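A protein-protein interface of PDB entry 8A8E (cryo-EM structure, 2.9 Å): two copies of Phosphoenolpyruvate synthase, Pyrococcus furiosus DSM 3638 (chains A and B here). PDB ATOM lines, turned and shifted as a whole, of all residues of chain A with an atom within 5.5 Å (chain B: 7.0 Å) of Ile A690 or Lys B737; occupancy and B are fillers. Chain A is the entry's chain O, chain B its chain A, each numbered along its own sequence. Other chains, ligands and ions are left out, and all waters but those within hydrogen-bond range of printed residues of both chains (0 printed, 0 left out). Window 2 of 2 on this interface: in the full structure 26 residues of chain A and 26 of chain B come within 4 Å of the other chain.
N of Ala A687 lies within hydrogen-bond range of O of Thr B714, 3.4 Å away. The backbone carbonyl oxygen of Ile A690 is in hydrogen-bond range of the side-chain amino group of Lys B737, 3.3 Å away.
A ring nitrogen (ND1) of His B732 lies within hydrogen-bond range of the backbone NH of Ala B734, at 3.2 Å.
Of the printed residues of chain B, Pro A686 touches Thr B714 (3.8 Å). Of the printed residues of chain B, Ala A687 touches Thr B714. Of the printed residues of chain B, Ile A690 touches Lys B737. Printed residues of chain B within 4 Å of Ile A691: His B732. His A741 touches none of the printed residues of chain B. Printed residues of chain A within 4 Å of His B732: Ile A691. Lys B737 touches just one residue of chain A: Ile A690.
Of the 9 printed residues of chain A, 4 touch a printed residue of chain B. Hydrophobic or aromatic side chains of chain A that line the printed part of chain B: Pro A686, Ala A687 and Ile A691. Hydrophobic or aromatic side chains of chain B within 4 Å of the printed part of chain A: His B732. Among the printed residues, 4 pairs touch across the chains.
Pro A686 touches Thr B714. Ile A691 touches His B732 (CD1 to CE1, 3.9 Å).
4 positions are printed for both chains. Of the 4 pairs that touch across the chains among the printed residues, none has its exchanged pair printed and touching as well.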
ATOM      1  N   PRO A 686      -2.236 -11.477 -18.565  1.00  0.00           N
ATOM      2  CA  PRO A 686      -0.788 -11.233 -18.652  1.00  0.00           C
ATOM      3  C   PRO A 686       0.000 -11.734 -17.455  1.00  0.00           C
ATOM      4  O   PRO A 686       1.159 -12.145 -17.611  1.00  0.00           O
ATOM      5  CB  PRO A 686      -0.714  -9.709 -18.785  1.00  0.00           C
ATOM      6  CG  PRO A 686      -1.982  -9.345 -19.445  1.00  0.00           C
ATOM      7  CD  PRO A 686      -3.016 -10.282 -18.919  1.00  0.00           C
ATOM      8  N   ALA A 687      -0.600 -11.731 -16.265  1.00  0.00           N
ATOM      9  CA  ALA A 687       0.092 -12.227 -15.082  1.00  0.00           C
ATOM     10  C   ALA A 687       0.505 -13.681 -15.254  1.00  0.00           C
ATOM     11  O   ALA A 687       1.628 -14.061 -14.914  1.00  0.00           O
ATOM     12  CB  ALA A 687      -0.791 -12.057 -13.848  1.00  0.00           C
ATOM     13  N   ALA A 688      -0.388 -14.511 -15.794  1.00  0.00           N
ATOM     14  CA  ALA A 688      -0.059 -15.920 -15.985  1.00  0.00           C
ATOM     15  C   ALA A 688       1.085 -16.091 -16.974  1.00  0.00           C
ATOM     16  O   ALA A 688       1.927 -16.978 -16.811  1.00  0.00           O
ATOM     17  CB  ALA A 688      -1.290 -16.690 -16.452  1.00  0.00           C
ATOM     18  N   ALA A 689       1.139 -15.244 -17.998  1.00  0.00           N
ATOM     19  CA  ALA A 689       2.238 -15.297 -18.949  1.00  0.00           C
ATOM     20  C   ALA A 689       3.551 -14.792 -18.363  1.00  0.00           C
ATOM     21  O   ALA A 689       4.611 -15.142 -18.882  1.00  0.00           O
ATOM     22  CB  ALA A 689       1.887 -14.494 -20.201  1.00  0.00           C
ATOM     23  N   ILE A 690       3.513 -13.984 -17.304  1.00  0.00           N
ATOM     24  CA  ILE A 690       4.752 -13.426 -16.763  1.00  0.00           C
ATOM     25  C   ILE A 690       5.364 -14.275 -15.639  1.00  0.00           C
ATOM     26  O   ILE A 690       6.578 -14.235 -15.431  1.00  0.00           O
ATOM     27  CB  ILE A 690       4.503 -11.973 -16.314  1.00  0.00           C
ATOM     28  CG1 ILE A 690       4.101 -11.123 -17.514  1.00  0.00           C
ATOM     29  CG2 ILE A 690       5.729 -11.360 -15.686  1.00  0.00           C
ATOM     30  CD1 ILE A 690       3.605  -9.753 -17.163  1.00  0.00           C
ATOM     31  N   ILE A 691       4.566 -15.067 -14.922  1.00  0.00           N
ATOM     32  CA  ILE A 691       5.083 -15.912 -13.844  1.00  0.00           C
ATOM     33  C   ILE A 691       4.869 -17.385 -14.163  1.00  0.00           C
ATOM     34  O   ILE A 691       4.583 -18.184 -13.266  1.00  0.00           O
ATOM     35  CB  ILE A 691       4.438 -15.572 -12.486  1.00  0.00           C
ATOM     36  CG1 ILE A 691       2.914 -15.582 -12.596  1.00  0.00           C
ATOM     37  CG2 ILE A 691       4.963 -14.248 -11.952  1.00  0.00           C
ATOM     38  CD1 ILE A 691       2.205 -15.529 -11.280  1.00  0.00           C
ATOM     39  N   ILE A 692       4.990 -17.750 -15.442  1.00  0.00           N
ATOM     40  CA  ILE A 692       4.609 -19.082 -15.914  1.00  0.00           C
ATOM     41  C   ILE A 692       5.339 -20.193 -15.165  1.00  0.00           C
ATOM     42  O   ILE A 692       4.797 -21.291 -14.985  1.00  0.00           O
ATOM     43  CB  ILE A 692       4.843 -19.160 -17.438  1.00  0.00           C
ATOM     44  CG1 ILE A 692       4.657 -20.584 -17.959  1.00  0.00           C
ATOM     45  CG2 ILE A 692       6.211 -18.604 -17.799  1.00  0.00           C
ATOM     46  CD1 ILE A 692       3.234 -21.062 -17.911  1.00  0.00           C
ATOM     47  N   LEU A 738       5.490 -11.921 -25.169  1.00  0.00           N
ATOM     48  CA  LEU A 738       4.957 -12.790 -24.122  1.00  0.00           C
ATOM     49  C   LEU A 738       4.906 -14.244 -24.576  1.00  0.00           C
ATOM     50  O   LEU A 738       5.289 -15.159 -23.828  1.00  0.00           O
ATOM     51  CB  LEU A 738       3.566 -12.313 -23.709  1.00  0.00           C
ATOM     52  CG  LEU A 738       3.423 -11.074 -22.825  1.00  0.00           C
ATOM     53  CD1 LEU A 738       1.962 -10.811 -22.562  1.00  0.00           C
ATOM     54  CD2 LEU A 738       4.178 -11.233 -21.521  1.00  0.00           C
ATOM     55  N   HIS A 741       8.431 -15.806 -24.655  1.00  0.00           N
ATOM     56  CA  HIS A 741       8.906 -16.142 -23.313  1.00  0.00           C
ATOM     57  C   HIS A 741       8.278 -17.440 -22.814  1.00  0.00           C
ATOM     58  O   HIS A 741       8.981 -18.347 -22.333  1.00  0.00           O
ATOM     59  CB  HIS A 741       8.607 -14.984 -22.359  1.00  0.00           C
ATOM     60  CG  HIS A 741       8.965 -15.258 -20.932  1.00  0.00           C
ATOM     61  ND1 HIS A 741      10.240 -15.588 -20.534  1.00  0.00           N
ATOM     62  CD2 HIS A 741       8.212 -15.241 -19.808  1.00  0.00           C
ATOM     63  CE1 HIS A 741      10.256 -15.778 -19.229  1.00  0.00           C
ATOM     64  NE2 HIS A 741       9.038 -15.571 -18.763  1.00  0.00           N
ATOM     65  N   PRO B 686      -0.213  -2.639 -19.671  1.00  0.00           N
ATOM     66  CA  PRO B 686       0.973  -3.505 -19.742  1.00  0.00           C
ATOM     67  C   PRO B 686       1.760  -3.376 -21.034  1.00  0.00           C
ATOM     68  O   PRO B 686       2.990  -3.530 -21.022  1.00  0.00           O
ATOM     69  CB  PRO B 686       0.374  -4.905 -19.577  1.00  0.00           C
ATOM     70  CG  PRO B 686      -0.839  -4.683 -18.768  1.00  0.00           C
ATOM     71  CD  PRO B 686      -1.399  -3.369 -19.198  1.00  0.00           C
ATOM     72  N   ILE B 690       5.865  -2.928 -21.643  1.00  0.00           N
ATOM     73  CA  ILE B 690       6.655  -3.965 -22.307  1.00  0.00           C
ATOM     74  C   ILE B 690       7.449  -3.448 -23.516  1.00  0.00           C
ATOM     75  O   ILE B 690       8.485  -4.020 -23.859  1.00  0.00           O
ATOM     76  CB  ILE B 690       5.734  -5.142 -22.686  1.00  0.00           C
ATOM     77  CG1 ILE B 690       5.135  -5.755 -21.425  1.00  0.00           C
ATOM     78  CG2 ILE B 690       6.477  -6.220 -23.432  1.00  0.00           C
ATOM     79  CD1 ILE B 690       4.043  -6.749 -21.680  1.00  0.00           C
ATOM     80  N   THR B 714      -3.338  -5.829 -15.227  1.00  0.00           N
ATOM     81  CA  THR B 714      -2.426  -6.960 -15.312  1.00  0.00           C
ATOM     82  C   THR B 714      -3.046  -8.237 -14.759  1.00  0.00           C
ATOM     83  O   THR B 714      -2.805  -9.321 -15.300  1.00  0.00           O
ATOM     84  CB  THR B 714      -1.127  -6.623 -14.579  1.00  0.00           C
ATOM     85  OG1 THR B 714      -0.511  -5.497 -15.210  1.00  0.00           O
ATOM     86  CG2 THR B 714      -0.166  -7.789 -14.614  1.00  0.00           C
ATOM     87  N   HIS B 732       2.332  -7.676  -6.104  1.00  0.00           N
ATOM     88  CA  HIS B 732       2.342  -8.961  -6.782  1.00  0.00           C
ATOM     89  C   HIS B 732       3.589  -9.070  -7.660  1.00  0.00           C
ATOM     90  O   HIS B 732       3.998  -8.084  -8.276  1.00  0.00           O
ATOM     91  CB  HIS B 732       1.071  -9.102  -7.620  1.00  0.00           C
ATOM     92  CG  HIS B 732       0.898 -10.440  -8.265  1.00  0.00           C
ATOM     93  ND1 HIS B 732       1.572 -10.810  -9.408  1.00  0.00           N
ATOM     94  CD2 HIS B 732       0.100 -11.486  -7.946  1.00  0.00           C
ATOM     95  CE1 HIS B 732       1.213 -12.031  -9.754  1.00  0.00           C
ATOM     96  NE2 HIS B 732       0.320 -12.465  -8.884  1.00  0.00           N
ATOM     97  N   PRO B 733       4.210 -10.252  -7.734  1.00  0.00           N
ATOM     98  CA  PRO B 733       5.483 -10.388  -8.471  1.00  0.00           C
ATOM     99  C   PRO B 733       5.480  -9.862  -9.901  1.00  0.00           C
ATOM    100  O   PRO B 733       6.519  -9.374 -10.371  1.00  0.00           O
ATOM    101  CB  PRO B 733       5.729 -11.900  -8.440  1.00  0.00           C
ATOM    102  CG  PRO B 733       5.004 -12.381  -7.249  1.00  0.00           C
ATOM    103  CD  PRO B 733       3.858 -11.472  -6.992  1.00  0.00           C
ATOM    104  N   ALA B 734       4.360  -9.947 -10.616  1.00  0.00           N
ATOM    105  CA  ALA B 734       4.370  -9.554 -12.021  1.00  0.00           C
ATOM    106  C   ALA B 734       4.511  -8.044 -12.178  1.00  0.00           C
ATOM    107  O   ALA B 734       5.286  -7.566 -13.021  1.00  0.00           O
ATOM    108  CB  ALA B 734       3.103 -10.053 -12.708  1.00  0.00           C
ATOM    109  N   VAL B 735       3.771  -7.282 -11.372  1.00  0.00           N
ATOM    110  CA  VAL B 735       3.878  -5.828 -11.404  1.00  0.00           C
ATOM    111  C   VAL B 735       5.296  -5.392 -11.059  1.00  0.00           C
ATOM    112  O   VAL B 735       5.834  -4.446 -11.651  1.00  0.00           O
ATOM    113  CB  VAL B 735       2.834  -5.207 -10.458  1.00  0.00           C
ATOM    114  CG1 VAL B 735       2.954  -3.697 -10.441  1.00  0.00           C
ATOM    115  CG2 VAL B 735       1.435  -5.615 -10.876  1.00  0.00           C
ATOM    116  N   LEU B 736       5.936  -6.090 -10.121  1.00  0.00           N
ATOM    117  CA  LEU B 736       7.289  -5.726  -9.719  1.00  0.00           C
ATOM    118  C   LEU B 736       8.296  -6.023 -10.822  1.00  0.00           C
ATOM    119  O   LEU B 736       9.225  -5.235 -11.044  1.00  0.00           O
ATOM    120  CB  LEU B 736       7.667  -6.457  -8.436  1.00  0.00           C
ATOM    121  CG  LEU B 736       6.913  -6.087  -7.156  1.00  0.00           C
ATOM    122  CD1 LEU B 736       7.626  -6.643  -5.949  1.00  0.00           C
ATOM    123  CD2 LEU B 736       6.732  -4.587  -7.022  1.00  0.00           C
ATOM    124  N   LYS B 737       8.133  -7.149 -11.522  1.00  0.00           N
ATOM    125  CA  LYS B 737       8.958  -7.414 -12.698  1.00  0.00           C
ATOM    126  C   LYS B 737       8.828  -6.297 -13.730  1.00  0.00           C
ATOM    127  O   LYS B 737       9.830  -5.822 -14.285  1.00  0.00           O
ATOM    128  CB  LYS B 737       8.566  -8.750 -13.319  1.00  0.00           C
ATOM    129  CG  LYS B 737       8.988  -9.959 -12.531  1.00  0.00           C
ATOM    130  CD  LYS B 737       9.509 -11.023 -13.456  1.00  0.00           C
ATOM    131  CE  LYS B 737       9.369 -12.390 -12.844  1.00  0.00           C
ATOM    132  NZ  LYS B 737       9.331 -13.432 -13.897  1.00  0.00           N
ATOM    133  N   LEU B 738       7.594  -5.866 -14.002  1.00  0.00           N
ATOM    134  CA  LEU B 738       7.389  -4.823 -15.005  1.00  0.00           C
ATOM    135  C   LEU B 738       8.045  -3.512 -14.587  1.00  0.00           C
ATOM    136  O   LEU B 738       8.708  -2.844 -15.398  1.00  0.00           O
ATOM    137  CB  LEU B 738       5.895  -4.618 -15.243  1.00  0.00           C
ATOM    138  CG  LEU B 738       5.115  -5.639 -16.072  1.00  0.00           C
ATOM    139  CD1 LEU B 738       3.670  -5.215 -16.160  1.00  0.00           C
ATOM    140  CD2 LEU B 738       5.707  -5.798 -17.457  1.00  0.00           C
ATOM    141  N   ILE B 739       7.875  -3.132 -13.318  1.00  0.00           N
ATOM    142  CA  ILE B 739       8.458  -1.893 -12.808  1.00  0.00           C
ATOM    143  C   ILE B 739       9.980  -1.939 -12.889  1.00  0.00           C
ATOM    144  O   ILE B 739      10.627  -0.962 -13.289  1.00  0.00           O
ATOM    145  CB  ILE B 739       7.969  -1.642 -11.370  1.00  0.00           C
ATOM    146  CG1 ILE B 739       6.480  -1.285 -11.362  1.00  0.00           C
ATOM    147  CG2 ILE B 739       8.785  -0.563 -10.698  1.00  0.00           C
ATOM    148  CD1 ILE B 739       5.874  -1.186  -9.986  1.00  0.00           C
ATOM    149  N   LYS B 740      10.576  -3.072 -12.508  1.00  0.00           N
ATOM    150  CA  LYS B 740      12.028  -3.206 -12.559  1.00  0.00           C
ATOM    151  C   LYS B 740      12.552  -3.059 -13.983  1.00  0.00           C
ATOM    152  O   LYS B 740      13.557  -2.372 -14.216  1.00  0.00           O
ATOM    153  CB  LYS B 740      12.432  -4.552 -11.963  1.00  0.00           C
ATOM    154  CG  LYS B 740      13.911  -4.762 -11.825  1.00  0.00           C
ATOM    155  CD  LYS B 740      14.204  -6.016 -11.035  1.00  0.00           C
ATOM    156  CE  LYS B 740      15.693  -6.244 -10.906  1.00  0.00           C
ATOM    157  NZ  LYS B 740      16.067  -6.664  -9.528  1.00  0.00           N
ATOM    158  N   HIS B 741      11.879  -3.689 -14.951  1.00  0.00           N
ATOM    159  CA  HIS B 741      12.298  -3.565 -16.347  1.00  0.00           C
ATOM    160  C   HIS B 741      12.264  -2.110 -16.806  1.00  0.00           C
ATOM    161  O   HIS B 741      13.237  -1.600 -17.388  1.00  0.00           O
ATOM    162  CB  HIS B 741      11.408  -4.442 -17.230  1.00  0.00           C
ATOM    163  CG  HIS B 741      11.686  -4.318 -18.694  1.00  0.00           C
ATOM    164  ND1 HIS B 741      12.919  -4.581 -19.244  1.00  0.00           N
ATOM    165  CD2 HIS B 741      10.882  -3.966 -19.725  1.00  0.00           C
ATOM    166  CE1 HIS B 741      12.870  -4.383 -20.547  1.00  0.00           C
ATOM    167  NE2 HIS B 741      11.644  -4.012 -20.866  1.00  0.00           N
ATOM    168  N   VAL B 742      11.146  -1.423 -16.549  1.00  0.00           N
ATOM    169  CA  VAL B 742      11.022  -0.035 -16.992  1.00  0.00           C
ATOM    170  C   VAL B 742      12.128   0.826 -16.386  1.00  0.00           C
ATOM    171  O   VAL B 742      12.796   1.597 -17.094  1.00  0.00           O
ATOM    172  CB  VAL B 742       9.631   0.524 -16.649  1.00  0.00           C
ATOM    173  CG1 VAL B 742       9.618   2.028 -16.831  1.00  0.00           C
ATOM    174  CG2 VAL B 742       8.573  -0.108 -17.518  1.00  0.00           C
